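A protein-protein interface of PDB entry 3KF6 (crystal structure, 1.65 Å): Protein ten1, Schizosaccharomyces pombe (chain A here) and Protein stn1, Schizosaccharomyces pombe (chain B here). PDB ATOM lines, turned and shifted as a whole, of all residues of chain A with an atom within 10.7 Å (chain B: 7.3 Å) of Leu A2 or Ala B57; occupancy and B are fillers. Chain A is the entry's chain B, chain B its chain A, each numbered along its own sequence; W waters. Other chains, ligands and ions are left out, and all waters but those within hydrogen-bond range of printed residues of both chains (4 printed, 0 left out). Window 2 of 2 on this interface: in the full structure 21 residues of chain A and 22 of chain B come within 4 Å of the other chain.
Leu A2 touches Ala B57. O of Ser A4 touches CG2 of Val B77, 3.7 Å away. Ala A7 touches Tyr B55. Val A69 touches Tyr B55. Tyr B55 touches Leu A82 (CE2 to CD1, 3.7 Å). CD2 of Leu A82 touches O of Pro B99 (3.9 Å). Leu A82 touches Gly B100. Gly B100 touches Arg A84.
NH2 of Arg A84 is in hydrogen-bond range of O of Pro B99 (3.0 Å). The side-chain carboxylate (OD1) of Asp B71 lies within hydrogen-bond range of the side-chain hydroxyl (OG) of Ser A6, at 2.7 Å. The side-chain amide oxygen (OD1) of Asn B101 is in hydrogen-bond range of the guanidinium group (NH2) of Arg A84. The side-chain carboxylate (OD2) of Asp B71 lies within hydrogen-bond range of the backbone NH (N) of Ala A7, at 2.9 Å.
Of the 15 printed residues of chain B, 7 touch a printed residue of chain A. Hydrophobic or aromatic side chains of chain B that line the printed part of chain A: Tyr B55 and Val B77. Among the printed residues, 12 pairs touch across the chains.
The backbone NH (N) of Ala B57 is in hydrogen-bond range of the backbone carbonyl oxygen (O) of Thr B69 (2.7 Å). N of Leu A81 lies within hydrogen-bond range of O of Val A69 (2.8 Å). The backbone carbonyl oxygen (O) of Leu A2 lies within hydrogen-bond range of the side-chain amino group (NZ) of Lys A23 (2.6 Å). O of Leu A2 lies within hydrogen-bond range of NH2 of Arg A71 (3.1 Å). The side-chain hydroxyl (OH) of Tyr B55 is in hydrogen-bond range of the side-chain carboxylate (OD2) of Asp B71. The backbone carbonyl oxygen (O) of Asn B101 sits at hydrogen-bond distance from the backbone NH (N) of Ile B56 (2.8 Å).
Water W4 bridges NZ of Lys A23 (2.7 Å) and OH of Tyr B55 (2.8 Å). Water W3 lies within hydrogen-bond range of the backbone carbonyl oxygen (O) of Ser A4 and the backbone NH (N) of Val B77. Water W1 bridges NH1 of Arg A25 and O of Asp B71. Water W2 lies within hydrogen-bond range of NH1 of Arg A84 (2.8 Å) and O of Pro B99 (3.3 Å).
Of chain B, only Ala B57 comes within 4 Å of Leu A2. Ala B57 touches one residue of chain A. No residue of chain B comes within 4 Å of Gly A3. No residue of chain A comes within 4 Å of Ile B56. No residue of chain A comes within 4 Å of Ala B58. No residue of chain A comes within 4 Å of Val B70. Of the printed residues of chain A, Tyr B55 touches Ala A7, Val A69 and Leu A82. Of the printed residues of chain A, Asp B71 touches Ser A6 (2.7 Å) and Ala A7 (2.9 Å). Of the printed residues of chain B, Leu A82 touches Tyr B55 (3.7 Å), Pro B99 (3.9 Å) and Gly B100 (3.9 Å). The nearest residue of chain B that does not touch Leu A2 is Ile B56 (4.1 Å). The nearest residue of chain A that does not touch Ala B57 is Gly A3 (4.8 Å). The nearest printed residue of chain A that does not touch Asp B71 is Asp A5 (4.2 Å).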
ATOM      1  N   PRO A   1     -21.744  26.103 -17.874  1.00  0.00           N
ATOM      2  CA  PRO A   1     -20.840  27.270 -17.982  1.00  0.00           C
ATOM      3  C   PRO A   1     -19.905  27.376 -16.782  1.00  0.00           C
ATOM      4  O   PRO A   1     -18.870  28.043 -16.843  1.00  0.00           O
ATOM      5  CB  PRO A   1     -21.724  28.501 -18.088  1.00  0.00           C
ATOM      6  CG  PRO A   1     -22.980  27.905 -18.725  1.00  0.00           C
ATOM      7  CD  PRO A   1     -23.143  26.532 -18.055  1.00  0.00           C
ATOM      8  N   LEU A   2     -20.279  26.719 -15.691  1.00  0.00           N
ATOM      9  CA  LEU A   2     -19.468  26.738 -14.485  1.00  0.00           C
ATOM     10  C   LEU A   2     -18.358  25.692 -14.537  1.00  0.00           C
ATOM     11  O   LEU A   2     -17.298  25.878 -13.950  1.00  0.00           O
ATOM     12  CB  LEU A   2     -20.342  26.484 -13.257  1.00  0.00           C
ATOM     13  CG  LEU A   2     -21.427  27.502 -12.908  1.00  0.00           C
ATOM     14  CD1 LEU A   2     -22.134  27.077 -11.633  1.00  0.00           C
ATOM     15  CD2 LEU A   2     -20.796  28.867 -12.724  1.00  0.00           C
ATOM     16  N   GLY A   3     -18.607  24.595 -15.243  1.00  0.00           N
ATOM     17  CA  GLY A   3     -17.617  23.538 -15.325  1.00  0.00           C
ATOM     18  C   GLY A   3     -17.892  22.568 -14.198  1.00  0.00           C
ATOM     19  O   GLY A   3     -18.566  22.924 -13.234  1.00  0.00           O
ATOM     20  N   SER A   4     -17.364  21.356 -14.302  1.00  0.00           N
ATOM     21  CA  SER A   4     -17.596  20.339 -13.288  1.00  0.00           C
ATOM     22  C   SER A   4     -16.568  20.333 -12.166  1.00  0.00           C
ATOM     23  O   SER A   4     -16.628  19.487 -11.281  1.00  0.00           O
ATOM     24  CB  SER A   4     -17.638  18.956 -13.946  1.00  0.00           C
ATOM     25  OG  SER A   4     -18.638  18.912 -14.949  1.00  0.00           O
ATOM     26  N   ASP A   5     -15.628  21.269 -12.191  1.00  0.00           N
ATOM     27  CA  ASP A   5     -14.616  21.313 -11.144  1.00  0.00           C
ATOM     28  C   ASP A   5     -15.158  21.971  -9.881  1.00  0.00           C
ATOM     29  O   ASP A   5     -16.033  22.836  -9.948  1.00  0.00           O
ATOM     30  CB  ASP A   5     -13.348  22.034 -11.643  1.00  0.00           C
ATOM     31  CG  ASP A   5     -13.634  23.408 -12.250  1.00  0.00           C
ATOM     32  OD1 ASP A   5     -14.663  23.574 -12.927  1.00  0.00           O
ATOM     33  OD2 ASP A   5     -12.803  24.321 -12.068  1.00  0.00           O
ATOM     34  N   SER A   6     -14.646  21.530  -8.736  1.00  0.00           N
ATOM     35  CA  SER A   6     -15.059  22.050  -7.436  1.00  0.00           C
ATOM     36  C   SER A   6     -14.248  23.291  -7.088  1.00  0.00           C
ATOM     37  O   SER A   6     -13.035  23.330  -7.284  1.00  0.00           O
ATOM     38  CB  SER A   6     -14.852  20.974  -6.364  1.00  0.00           C
ATOM     39  OG  SER A   6     -15.215  21.451  -5.079  1.00  0.00           O
ATOM     40  N   ALA A   7     -14.925  24.307  -6.563  1.00  0.00           N
ATOM     41  CA  ALA A   7     -14.253  25.545  -6.199  1.00  0.00           C
ATOM     42  C   ALA A   7     -13.404  25.412  -4.935  1.00  0.00           C
ATOM     43  O   ALA A   7     -13.720  24.627  -4.031  1.00  0.00           O
ATOM     44  CB  ALA A   7     -15.291  26.658  -6.017  1.00  0.00           C
ATOM     45  N   LYS A   8     -12.298  26.151  -4.893  1.00  0.00           N
ATOM     46  CA  LYS A   8     -11.431  26.166  -3.718  1.00  0.00           C
ATOM     47  C   LYS A   8     -11.909  27.328  -2.861  1.00  0.00           C
ATOM     48  O   LYS A   8     -11.909  28.477  -3.311  1.00  0.00           O
ATOM     49  CB  LYS A   8      -9.969  26.404  -4.108  1.00  0.00           C
ATOM     50  CG  LYS A   8      -9.215  25.147  -4.491  1.00  0.00           C
ATOM     51  CD  LYS A   8      -7.795  25.475  -4.933  1.00  0.00           C
ATOM     52  CE  LYS A   8      -7.001  26.200  -3.854  1.00  0.00           C
ATOM     53  NZ  LYS A   8      -5.658  26.624  -4.369  1.00  0.00           N
ATOM     54  N   GLY A  21      -6.761  29.904 -13.884  1.00  0.00           N
ATOM     55  CA  GLY A  21      -7.693  28.939 -14.442  1.00  0.00           C
ATOM     56  C   GLY A  21      -8.412  28.144 -13.365  1.00  0.00           C
ATOM     57  O   GLY A  21      -9.392  27.453 -13.625  1.00  0.00           O
ATOM     58  N   GLN A  22      -7.917  28.254 -12.144  1.00  0.00           N
ATOM     59  CA  GLN A  22      -8.488  27.546 -11.009  1.00  0.00           C
ATOM     60  C   GLN A  22      -9.786  28.205 -10.547  1.00  0.00           C
ATOM     61  O   GLN A  22      -9.869  29.432 -10.462  1.00  0.00           O
ATOM     62  CB  GLN A  22      -7.455  27.551  -9.891  1.00  0.00           C
ATOM     63  CG  GLN A  22      -7.786  26.785  -8.650  1.00  0.00           C
ATOM     64  CD  GLN A  22      -6.615  26.806  -7.697  1.00  0.00           C
ATOM     65  OE1 GLN A  22      -5.554  26.253  -7.989  1.00  0.00           O
ATOM     66  NE2 GLN A  22      -6.788  27.469  -6.563  1.00  0.00           N
ATOM     67  N   LYS A  23     -10.805  27.394 -10.270  1.00  0.00           N
ATOM     68  CA  LYS A  23     -12.082  27.929  -9.797  1.00  0.00           C
ATOM     69  C   LYS A  23     -11.943  28.236  -8.313  1.00  0.00           C
ATOM     70  O   LYS A  23     -11.498  27.395  -7.540  1.00  0.00           O
ATOM     71  CB  LYS A  23     -13.208  26.924 -10.010  1.00  0.00           C
ATOM     72  CG  LYS A  23     -14.571  27.439  -9.542  1.00  0.00           C
ATOM     73  CD  LYS A  23     -15.679  26.415  -9.775  1.00  0.00           C
ATOM     74  CE  LYS A  23     -15.914  26.156 -11.253  1.00  0.00           C
ATOM     75  NZ  LYS A  23     -16.977  25.134 -11.485  1.00  0.00           N
ATOM     76  N   LEU A  24     -12.352  29.441  -7.919  1.00  0.00           N
ATOM     77  CA  LEU A  24     -12.224  29.874  -6.533  1.00  0.00           C
ATOM     78  C   LEU A  24     -13.528  30.425  -5.978  1.00  0.00           C
ATOM     79  O   LEU A  24     -14.335  30.978  -6.716  1.00  0.00           O
ATOM     80  CB  LEU A  24     -11.180  30.990  -6.433  1.00  0.00           C
ATOM     81  CG  LEU A  24      -9.831  30.793  -7.128  1.00  0.00           C
ATOM     82  CD1 LEU A  24      -9.052  32.110  -7.117  1.00  0.00           C
ATOM     83  CD2 LEU A  24      -9.056  29.693  -6.421  1.00  0.00           C
ATOM     84  N   ARG A  25     -13.727  30.266  -4.677  1.00  0.00           N
ATOM     85  CA  ARG A  25     -14.901  30.838  -4.030  1.00  0.00           C
ATOM     86  C   ARG A  25     -14.403  31.681  -2.862  1.00  0.00           C
ATOM     87  O   ARG A  25     -13.611  31.211  -2.041  1.00  0.00           O
ATOM     88  CB  ARG A  25     -15.870  29.769  -3.515  1.00  0.00           C
ATOM     89  CG  ARG A  25     -16.974  30.417  -2.685  1.00  0.00           C
ATOM     90  CD  ARG A  25     -17.958  29.438  -2.093  1.00  0.00           C
ATOM     91  NE  ARG A  25     -18.748  30.085  -1.046  1.00  0.00           N
ATOM     92  CZ  ARG A  25     -19.833  29.552  -0.492  1.00  0.00           C
ATOM     93  NH1 ARG A  25     -20.267  28.358  -0.887  1.00  0.00           N
ATOM     94  NH2 ARG A  25     -20.481  30.212   0.459  1.00  0.00           N
ATOM     95  N   VAL A  53     -19.835  39.745 -17.963  1.00  0.00           N
ATOM     96  CA  VAL A  53     -20.784  38.760 -18.473  1.00  0.00           C
ATOM     97  C   VAL A  53     -21.883  38.407 -17.474  1.00  0.00           C
ATOM     98  O   VAL A  53     -22.899  37.818 -17.841  1.00  0.00           O
ATOM     99  CB  VAL A  53     -20.084  37.443 -18.878  1.00  0.00           C
ATOM    100  CG1 VAL A  53     -19.034  37.713 -19.952  1.00  0.00           C
ATOM    101  CG2 VAL A  53     -19.458  36.774 -17.662  1.00  0.00           C
ATOM    102  N   VAL A  54     -21.688  38.769 -16.210  1.00  0.00           N
ATOM    103  CA  VAL A  54     -22.674  38.455 -15.182  1.00  0.00           C
ATOM    104  C   VAL A  54     -23.164  39.703 -14.443  1.00  0.00           C
ATOM    105  O   VAL A  54     -23.112  39.779 -13.215  1.00  0.00           O
ATOM    106  CB  VAL A  54     -22.094  37.427 -14.175  1.00  0.00           C
ATOM    107  CG1 VAL A  54     -20.887  38.018 -13.462  1.00  0.00           C
ATOM    108  CG2 VAL A  54     -23.167  36.995 -13.183  1.00  0.00           C
ATOM    109  N   ILE A  68     -18.460  35.196  -4.104  1.00  0.00           N
ATOM    110  CA  ILE A  68     -18.043  35.092  -5.493  1.00  0.00           C
ATOM    111  C   ILE A  68     -17.512  33.711  -5.845  1.00  0.00           C
ATOM    112  O   ILE A  68     -16.778  33.116  -5.068  1.00  0.00           O
ATOM    113  CB  ILE A  68     -16.881  36.087  -5.795  1.00  0.00           C
ATOM    114  CG1 ILE A  68     -17.347  37.530  -5.593  1.00  0.00           C
ATOM    115  CG2 ILE A  68     -16.359  35.890  -7.218  1.00  0.00           C
ATOM    116  CD1 ILE A  68     -18.382  37.985  -6.586  1.00  0.00           C
ATOM    117  N   VAL A  69     -17.916  33.205  -7.003  1.00  0.00           N
ATOM    118  CA  VAL A  69     -17.371  31.957  -7.523  1.00  0.00           C
ATOM    119  C   VAL A  69     -16.866  32.383  -8.891  1.00  0.00           C
ATOM    120  O   VAL A  69     -17.614  32.962  -9.678  1.00  0.00           O
ATOM    121  CB  VAL A  69     -18.415  30.843  -7.705  1.00  0.00           C
ATOM    122  CG1 VAL A  69     -17.753  29.641  -8.406  1.00  0.00           C
ATOM    123  CG2 VAL A  69     -18.957  30.411  -6.358  1.00  0.00           C
ATOM    124  N   GLY A  70     -15.591  32.137  -9.164  1.00  0.00           N
ATOM    125  CA  GLY A  70     -15.047  32.516 -10.452  1.00  0.00           C
ATOM    126  C   GLY A  70     -13.729  31.829 -10.713  1.00  0.00           C
ATOM    127  O   GLY A  70     -13.295  30.998  -9.919  1.00  0.00           O
ATOM    128  N   ARG A  71     -13.095  32.168 -11.830  1.00  0.00           N
ATOM    129  CA  ARG A  71     -11.808  31.580 -12.183  1.00  0.00           C
ATOM    130  C   ARG A  71     -10.719  32.637 -12.192  1.00  0.00           C
ATOM    131  O   ARG A  71     -10.923  33.749 -12.685  1.00  0.00           O
ATOM    132  CB  ARG A  71     -11.869  30.927 -13.566  1.00  0.00           C
ATOM    133  CG  ARG A  71     -12.733  29.696 -13.651  1.00  0.00           C
ATOM    134  CD  ARG A  71     -12.547  28.995 -14.996  1.00  0.00           C
ATOM    135  NE  ARG A  71     -13.456  27.865 -15.113  1.00  0.00           N
ATOM    136  CZ  ARG A  71     -13.335  26.736 -14.424  1.00  0.00           C
ATOM    137  NH1 ARG A  71     -12.329  26.577 -13.573  1.00  0.00           N
ATOM    138  NH2 ARG A  71     -14.239  25.778 -14.567  1.00  0.00           N
ATOM    139  N   LYS A  72      -9.560  32.289 -11.646  1.00  0.00           N
ATOM    140  CA  LYS A  72      -8.438  33.215 -11.614  1.00  0.00           C
ATOM    141  C   LYS A  72      -7.905  33.396 -13.032  1.00  0.00           C
ATOM    142  O   LYS A  72      -7.583  32.416 -13.708  1.00  0.00           O
ATOM    143  CB  LYS A  72      -7.334  32.670 -10.701  1.00  0.00           C
ATOM    144  CG  LYS A  72      -6.098  33.553 -10.592  1.00  0.00           C
ATOM    145  CD  LYS A  72      -5.214  33.086  -9.442  1.00  0.00           C
ATOM    146  CE  LYS A  72      -3.998  33.980  -9.241  1.00  0.00           C
ATOM    147  NZ  LYS A  72      -2.962  33.749 -10.279  1.00  0.00           N
ATOM    148  N   ASP A  79     -12.284  36.145 -13.041  1.00  0.00           N
ATOM    149  CA  ASP A  79     -13.414  36.186 -13.964  1.00  0.00           C
ATOM    150  C   ASP A  79     -14.596  35.576 -13.217  1.00  0.00           C
ATOM    151  O   ASP A  79     -14.609  34.379 -12.930  1.00  0.00           O
ATOM    152  CB  ASP A  79     -13.114  35.371 -15.227  1.00  0.00           C
ATOM    153  CG  ASP A  79     -12.283  36.140 -16.233  1.00  0.00           C
ATOM    154  OD1 ASP A  79     -12.736  37.218 -16.674  1.00  0.00           O
ATOM    155  OD2 ASP A  79     -11.181  35.669 -16.587  1.00  0.00           O
ATOM    156  N   VAL A  80     -15.590  36.401 -12.904  1.00  0.00           N
ATOM    157  CA  VAL A  80     -16.751  35.938 -12.150  1.00  0.00           C
ATOM    158  C   VAL A  80     -17.735  35.052 -12.899  1.00  0.00           C
ATOM    159  O   VAL A  80     -18.097  35.326 -14.046  1.00  0.00           O
ATOM    160  CB  VAL A  80     -17.531  37.133 -11.559  1.00  0.00           C
ATOM    161  CG1 VAL A  80     -18.714  36.630 -10.747  1.00  0.00           C
ATOM    162  CG2 VAL A  80     -16.605  37.974 -10.689  1.00  0.00           C
ATOM    163  N   LEU A  81     -18.177  33.991 -12.224  1.00  0.00           N
ATOM    164  CA  LEU A  81     -19.137  33.043 -12.779  1.00  0.00           C
ATOM    165  C   LEU A  81     -20.460  33.118 -12.017  1.00  0.00           C
ATOM    166  O   LEU A  81     -21.536  32.972 -12.596  1.00  0.00           O
ATOM    167  CB  LEU A  81     -18.585  31.614 -12.690  1.00  0.00           C
ATOM    168  CG  LEU A  81     -17.267  31.342 -13.421  1.00  0.00           C
ATOM    169  CD1 LEU A  81     -16.798  29.930 -13.117  1.00  0.00           C
ATOM    170  CD2 LEU A  81     -17.454  31.540 -14.910  1.00  0.00           C
ATOM    171  N   LEU A  82     -20.372  33.334 -10.708  1.00  0.00           N
ATOM    172  CA  LEU A  82     -21.560  33.436  -9.868  1.00  0.00           C
ATOM    173  C   LEU A  82     -21.388  34.505  -8.800  1.00  0.00           C
ATOM    174  O   LEU A  82     -20.309  34.652  -8.230  1.00  0.00           O
ATOM    175  CB  LEU A  82     -21.844  32.106  -9.166  1.00  0.00           C
ATOM    176  CG  LEU A  82     -22.190  30.869  -9.996  1.00  0.00           C
ATOM    177  CD1 LEU A  82     -22.234  29.660  -9.078  1.00  0.00           C
ATOM    178  CD2 LEU A  82     -23.527  31.065 -10.692  1.00  0.00           C
ATOM    179  N   ILE A  83     -22.462  35.244  -8.528  1.00  0.00           N
ATOM    180  CA  ILE A  83     -22.440  36.283  -7.506  1.00  0.00           C
ATOM    181  C   ILE A  83     -23.695  36.159  -6.645  1.00  0.00           C
ATOM    182  O   ILE A  83     -24.795  35.955  -7.162  1.00  0.00           O
ATOM    183  CB  ILE A  83     -22.454  37.705  -8.114  1.00  0.00           C
ATOM    184  CG1 ILE A  83     -21.353  37.857  -9.156  1.00  0.00           C
ATOM    185  CG2 ILE A  83     -22.270  38.742  -7.007  1.00  0.00           C
ATOM    186  CD1 ILE A  83     -21.412  39.191  -9.886  1.00  0.00           C
ATOM    187  N   ARG A  84     -23.530  36.280  -5.335  1.00  0.00           N
ATOM    188  CA  ARG A  84     -24.663  36.216  -4.416  1.00  0.00           C
ATOM    189  C   ARG A  84     -24.379  37.139  -3.242  1.00  0.00           C
ATOM    190  O   ARG A  84     -23.243  37.252  -2.799  1.00  0.00           O
ATOM    191  CB  ARG A  84     -24.873  34.793  -3.887  1.00  0.00           C
ATOM    192  CG  ARG A  84     -25.607  33.841  -4.827  1.00  0.00           C
ATOM    193  CD  ARG A  84     -27.086  34.215  -4.973  1.00  0.00           C
ATOM    194  NE  ARG A  84     -27.848  33.197  -5.693  1.00  0.00           N
ATOM    195  CZ  ARG A  84     -27.656  32.878  -6.968  1.00  0.00           C
ATOM    196  NH1 ARG A  84     -26.723  33.497  -7.679  1.00  0.00           N
ATOM    197  NH2 ARG A  84     -28.401  31.938  -7.535  1.00  0.00           N
ATOM    198  N   GLY B  54     -24.505  22.622  -0.283  1.00  0.00           N
ATOM    199  CA  GLY B  54     -23.630  23.301  -1.224  1.00  0.00           C
ATOM    200  C   GLY B  54     -24.422  24.101  -2.233  1.00  0.00           C
ATOM    201  O   GLY B  54     -25.651  24.119  -2.175  1.00  0.00           O
ATOM    202  N   TYR B  55     -23.739  24.775  -3.154  1.00  0.00           N
ATOM    203  CA  TYR B  55     -24.454  25.567  -4.153  1.00  0.00           C
ATOM    204  C   TYR B  55     -24.645  24.750  -5.427  1.00  0.00           C
ATOM    205  O   TYR B  55     -23.889  23.818  -5.699  1.00  0.00           O
ATOM    206  CB  TYR B  55     -23.710  26.881  -4.464  1.00  0.00           C
ATOM    207  CG  TYR B  55     -22.415  26.728  -5.237  1.00  0.00           C
ATOM    208  CD1 TYR B  55     -21.196  26.557  -4.573  1.00  0.00           C
ATOM    209  CD2 TYR B  55     -22.414  26.718  -6.633  1.00  0.00           C
ATOM    210  CE1 TYR B  55     -20.003  26.369  -5.288  1.00  0.00           C
ATOM    211  CE2 TYR B  55     -21.227  26.532  -7.355  1.00  0.00           C
ATOM    212  CZ  TYR B  55     -20.032  26.354  -6.674  1.00  0.00           C
ATOM    213  OH  TYR B  55     -18.877  26.115  -7.388  1.00  0.00           O
ATOM    214  N   ILE B  56     -25.671  25.101  -6.196  1.00  0.00           N
ATOM    215  CA  ILE B  56     -25.980  24.393  -7.432  1.00  0.00           C
ATOM    216  C   ILE B  56     -25.073  24.842  -8.564  1.00  0.00           C
ATOM    217  O   ILE B  56     -25.078  26.012  -8.953  1.00  0.00           O
ATOM    218  CB  ILE B  56     -27.450  24.621  -7.833  1.00  0.00           C
ATOM    219  CG1 ILE B  56     -28.367  24.015  -6.771  1.00  0.00           C
ATOM    220  CG2 ILE B  56     -27.731  23.980  -9.197  1.00  0.00           C
ATOM    221  CD1 ILE B  56     -29.819  24.386  -6.947  1.00  0.00           C
ATOM    222  N   ALA B  57     -24.297  23.903  -9.093  1.00  0.00           N
ATOM    223  CA  ALA B  57     -23.374  24.202 -10.174  1.00  0.00           C
ATOM    224  C   ALA B  57     -24.029  23.957 -11.521  1.00  0.00           C
ATOM    225  O   ALA B  57     -23.660  24.575 -12.521  1.00  0.00           O
ATOM    226  CB  ALA B  57     -22.120  23.346 -10.043  1.00  0.00           C
ATOM    227  N   ALA B  58     -25.001  23.054 -11.551  1.00  0.00           N
ATOM    228  CA  ALA B  58     -25.664  22.746 -12.805  1.00  0.00           C
ATOM    229  C   ALA B  58     -26.974  22.009 -12.610  1.00  0.00           C
ATOM    230  O   ALA B  58     -27.221  21.408 -11.566  1.00  0.00           O
ATOM    231  CB  ALA B  58     -24.735  21.921 -13.679  1.00  0.00           C
ATOM    232  N   ILE B  59     -27.816  22.074 -13.632  1.00  0.00           N
ATOM    233  CA  ILE B  59     -29.100  21.397 -13.615  1.00  0.00           C
ATOM    234  C   ILE B  59     -29.232  20.667 -14.945  1.00  0.00           C
ATOM    235  O   ILE B  59     -29.079  21.264 -16.011  1.00  0.00           O
ATOM    236  CB  ILE B  59     -30.263  22.397 -13.465  1.00  0.00           C
ATOM    237  CG1 ILE B  59     -30.083  23.204 -12.178  1.00  0.00           C
ATOM    238  CG2 ILE B  59     -31.593  21.650 -13.445  1.00  0.00           C
ATOM    239  CD1 ILE B  59     -31.068  24.346 -12.021  1.00  0.00           C
ATOM    240  N   LEU B  68     -29.337  17.684 -10.010  1.00  0.00           N
ATOM    241  CA  LEU B  68     -28.668  18.911  -9.606  1.00  0.00           C
ATOM    242  C   LEU B  68     -27.230  18.573  -9.225  1.00  0.00           C
ATOM    243  O   LEU B  68     -26.996  17.694  -8.397  1.00  0.00           O
ATOM    244  CB  LEU B  68     -29.362  19.535  -8.388  1.00  0.00           C
ATOM    245  CG  LEU B  68     -30.758  20.138  -8.542  1.00  0.00           C
ATOM    246  CD1 LEU B  68     -31.192  20.748  -7.221  1.00  0.00           C
ATOM    247  CD2 LEU B  68     -30.744  21.189  -9.629  1.00  0.00           C
ATOM    248  N   THR B  69     -26.267  19.254  -9.838  1.00  0.00           N
ATOM    249  CA  THR B  69     -24.875  19.020  -9.486  1.00  0.00           C
ATOM    250  C   THR B  69     -24.582  20.048  -8.397  1.00  0.00           C
ATOM    251  O   THR B  69     -24.773  21.249  -8.604  1.00  0.00           O
ATOM    252  CB  THR B  69     -23.931  19.240 -10.682  1.00  0.00           C
ATOM    253  OG1 THR B  69     -24.230  18.280 -11.706  1.00  0.00           O
ATOM    254  CG2 THR B  69     -22.480  19.054 -10.251  1.00  0.00           C
ATOM    255  N   VAL B  70     -24.126  19.571  -7.241  1.00  0.00           N
ATOM    256  CA  VAL B  70     -23.858  20.444  -6.099  1.00  0.00           C
ATOM    257  C   VAL B  70     -22.380  20.477  -5.737  1.00  0.00           C
ATOM    258  O   VAL B  70     -21.704  19.449  -5.766  1.00  0.00           O
ATOM    259  CB  VAL B  70     -24.679  19.976  -4.876  1.00  0.00           C
ATOM    260  CG1 VAL B  70     -24.421  20.885  -3.673  1.00  0.00           C
ATOM    261  CG2 VAL B  70     -26.170  19.973  -5.234  1.00  0.00           C
ATOM    262  N   ASP B  71     -21.892  21.667  -5.391  1.00  0.00           N
ATOM    263  CA  ASP B  71     -20.495  21.859  -5.020  1.00  0.00           C
ATOM    264  C   ASP B  71     -20.409  22.429  -3.609  1.00  0.00           C
ATOM    265  O   ASP B  71     -21.000  23.467  -3.331  1.00  0.00           O
ATOM    266  CB  ASP B  71     -19.833  22.836  -6.001  1.00  0.00           C
ATOM    267  CG  ASP B  71     -18.351  23.034  -5.729  1.00  0.00           C
ATOM    268  OD1 ASP B  71     -17.775  22.232  -4.971  1.00  0.00           O
ATOM    269  OD2 ASP B  71     -17.758  23.984  -6.291  1.00  0.00           O
ATOM    270  N   VAL B  77     -17.666  17.399  -6.752  1.00  0.00           N
ATOM    271  CA  VAL B  77     -19.071  17.800  -6.813  1.00  0.00           C
ATOM    272  C   VAL B  77     -19.894  16.515  -6.758  1.00  0.00           C
ATOM    273  O   VAL B  77     -19.367  15.422  -6.973  1.00  0.00           O
ATOM    274  CB  VAL B  77     -19.433  18.584  -8.100  1.00  0.00           C
ATOM    275  CG1 VAL B  77     -18.615  19.867  -8.177  1.00  0.00           C
ATOM    276  CG2 VAL B  77     -19.212  17.711  -9.335  1.00  0.00           C
ATOM    277  N   SER B  98     -31.955  27.804  -9.277  1.00  0.00           N
ATOM    278  CA  SER B  98     -31.063  28.404 -10.263  1.00  0.00           C
ATOM    279  C   SER B  98     -29.630  28.148  -9.826  1.00  0.00           C
ATOM    280  O   SER B  98     -29.360  27.999  -8.634  1.00  0.00           O
ATOM    281  CB  SER B  98     -31.279  29.919 -10.339  1.00  0.00           C
ATOM    282  OG  SER B  98     -32.617  30.240 -10.666  1.00  0.00           O
ATOM    283  N   PRO B  99     -28.695  28.081 -10.785  1.00  0.00           N
ATOM    284  CA  PRO B  99     -27.294  27.850 -10.421  1.00  0.00           C
ATOM    285  C   PRO B  99     -26.879  28.949  -9.447  1.00  0.00           C
ATOM    286  O   PRO B  99     -27.203  30.127  -9.649  1.00  0.00           O
ATOM    287  CB  PRO B  99     -26.569  27.963 -11.757  1.00  0.00           C
ATOM    288  CG  PRO B  99     -27.590  27.435 -12.727  1.00  0.00           C
ATOM    289  CD  PRO B  99     -28.860  28.115 -12.247  1.00  0.00           C
ATOM    290  N   GLY B 100     -26.175  28.567  -8.387  1.00  0.00           N
ATOM    291  CA  GLY B 100     -25.759  29.545  -7.399  1.00  0.00           C
ATOM    292  C   GLY B 100     -26.584  29.422  -6.130  1.00  0.00           C
ATOM    293  O   GLY B 100     -26.146  29.828  -5.056  1.00  0.00           O
ATOM    294  N   ASN B 101     -27.793  28.875  -6.240  1.00  0.00           N
ATOM    295  CA  ASN B 101     -28.625  28.702  -5.054  1.00  0.00           C
ATOM    296  C   ASN B 101     -27.968  27.657  -4.162  1.00  0.00           C
ATOM    297  O   ASN B 101     -27.346  26.714  -4.659  1.00  0.00           O
ATOM    298  CB  ASN B 101     -30.027  28.210  -5.423  1.00  0.00           C
ATOM    299  CG  ASN B 101     -30.850  29.257  -6.134  1.00  0.00           C
ATOM    300  OD1 ASN B 101     -30.435  30.404  -6.277  1.00  0.00           O
ATOM    301  ND2 ASN B 101     -32.042  28.862  -6.581  1.00  0.00           N
HETATM  302  O   HOH W   1     -20.104  25.649  -1.597  1.00  0.00           O
HETATM  303  O   HOH W   2     -27.245  33.291 -10.455  1.00  0.00           O
HETATM  304  O   HOH W   3     -15.464  17.741  -9.434  1.00  0.00           O
HETATM  305  O   HOH W   4     -19.244  25.443 -10.042  1.00  0.00           O
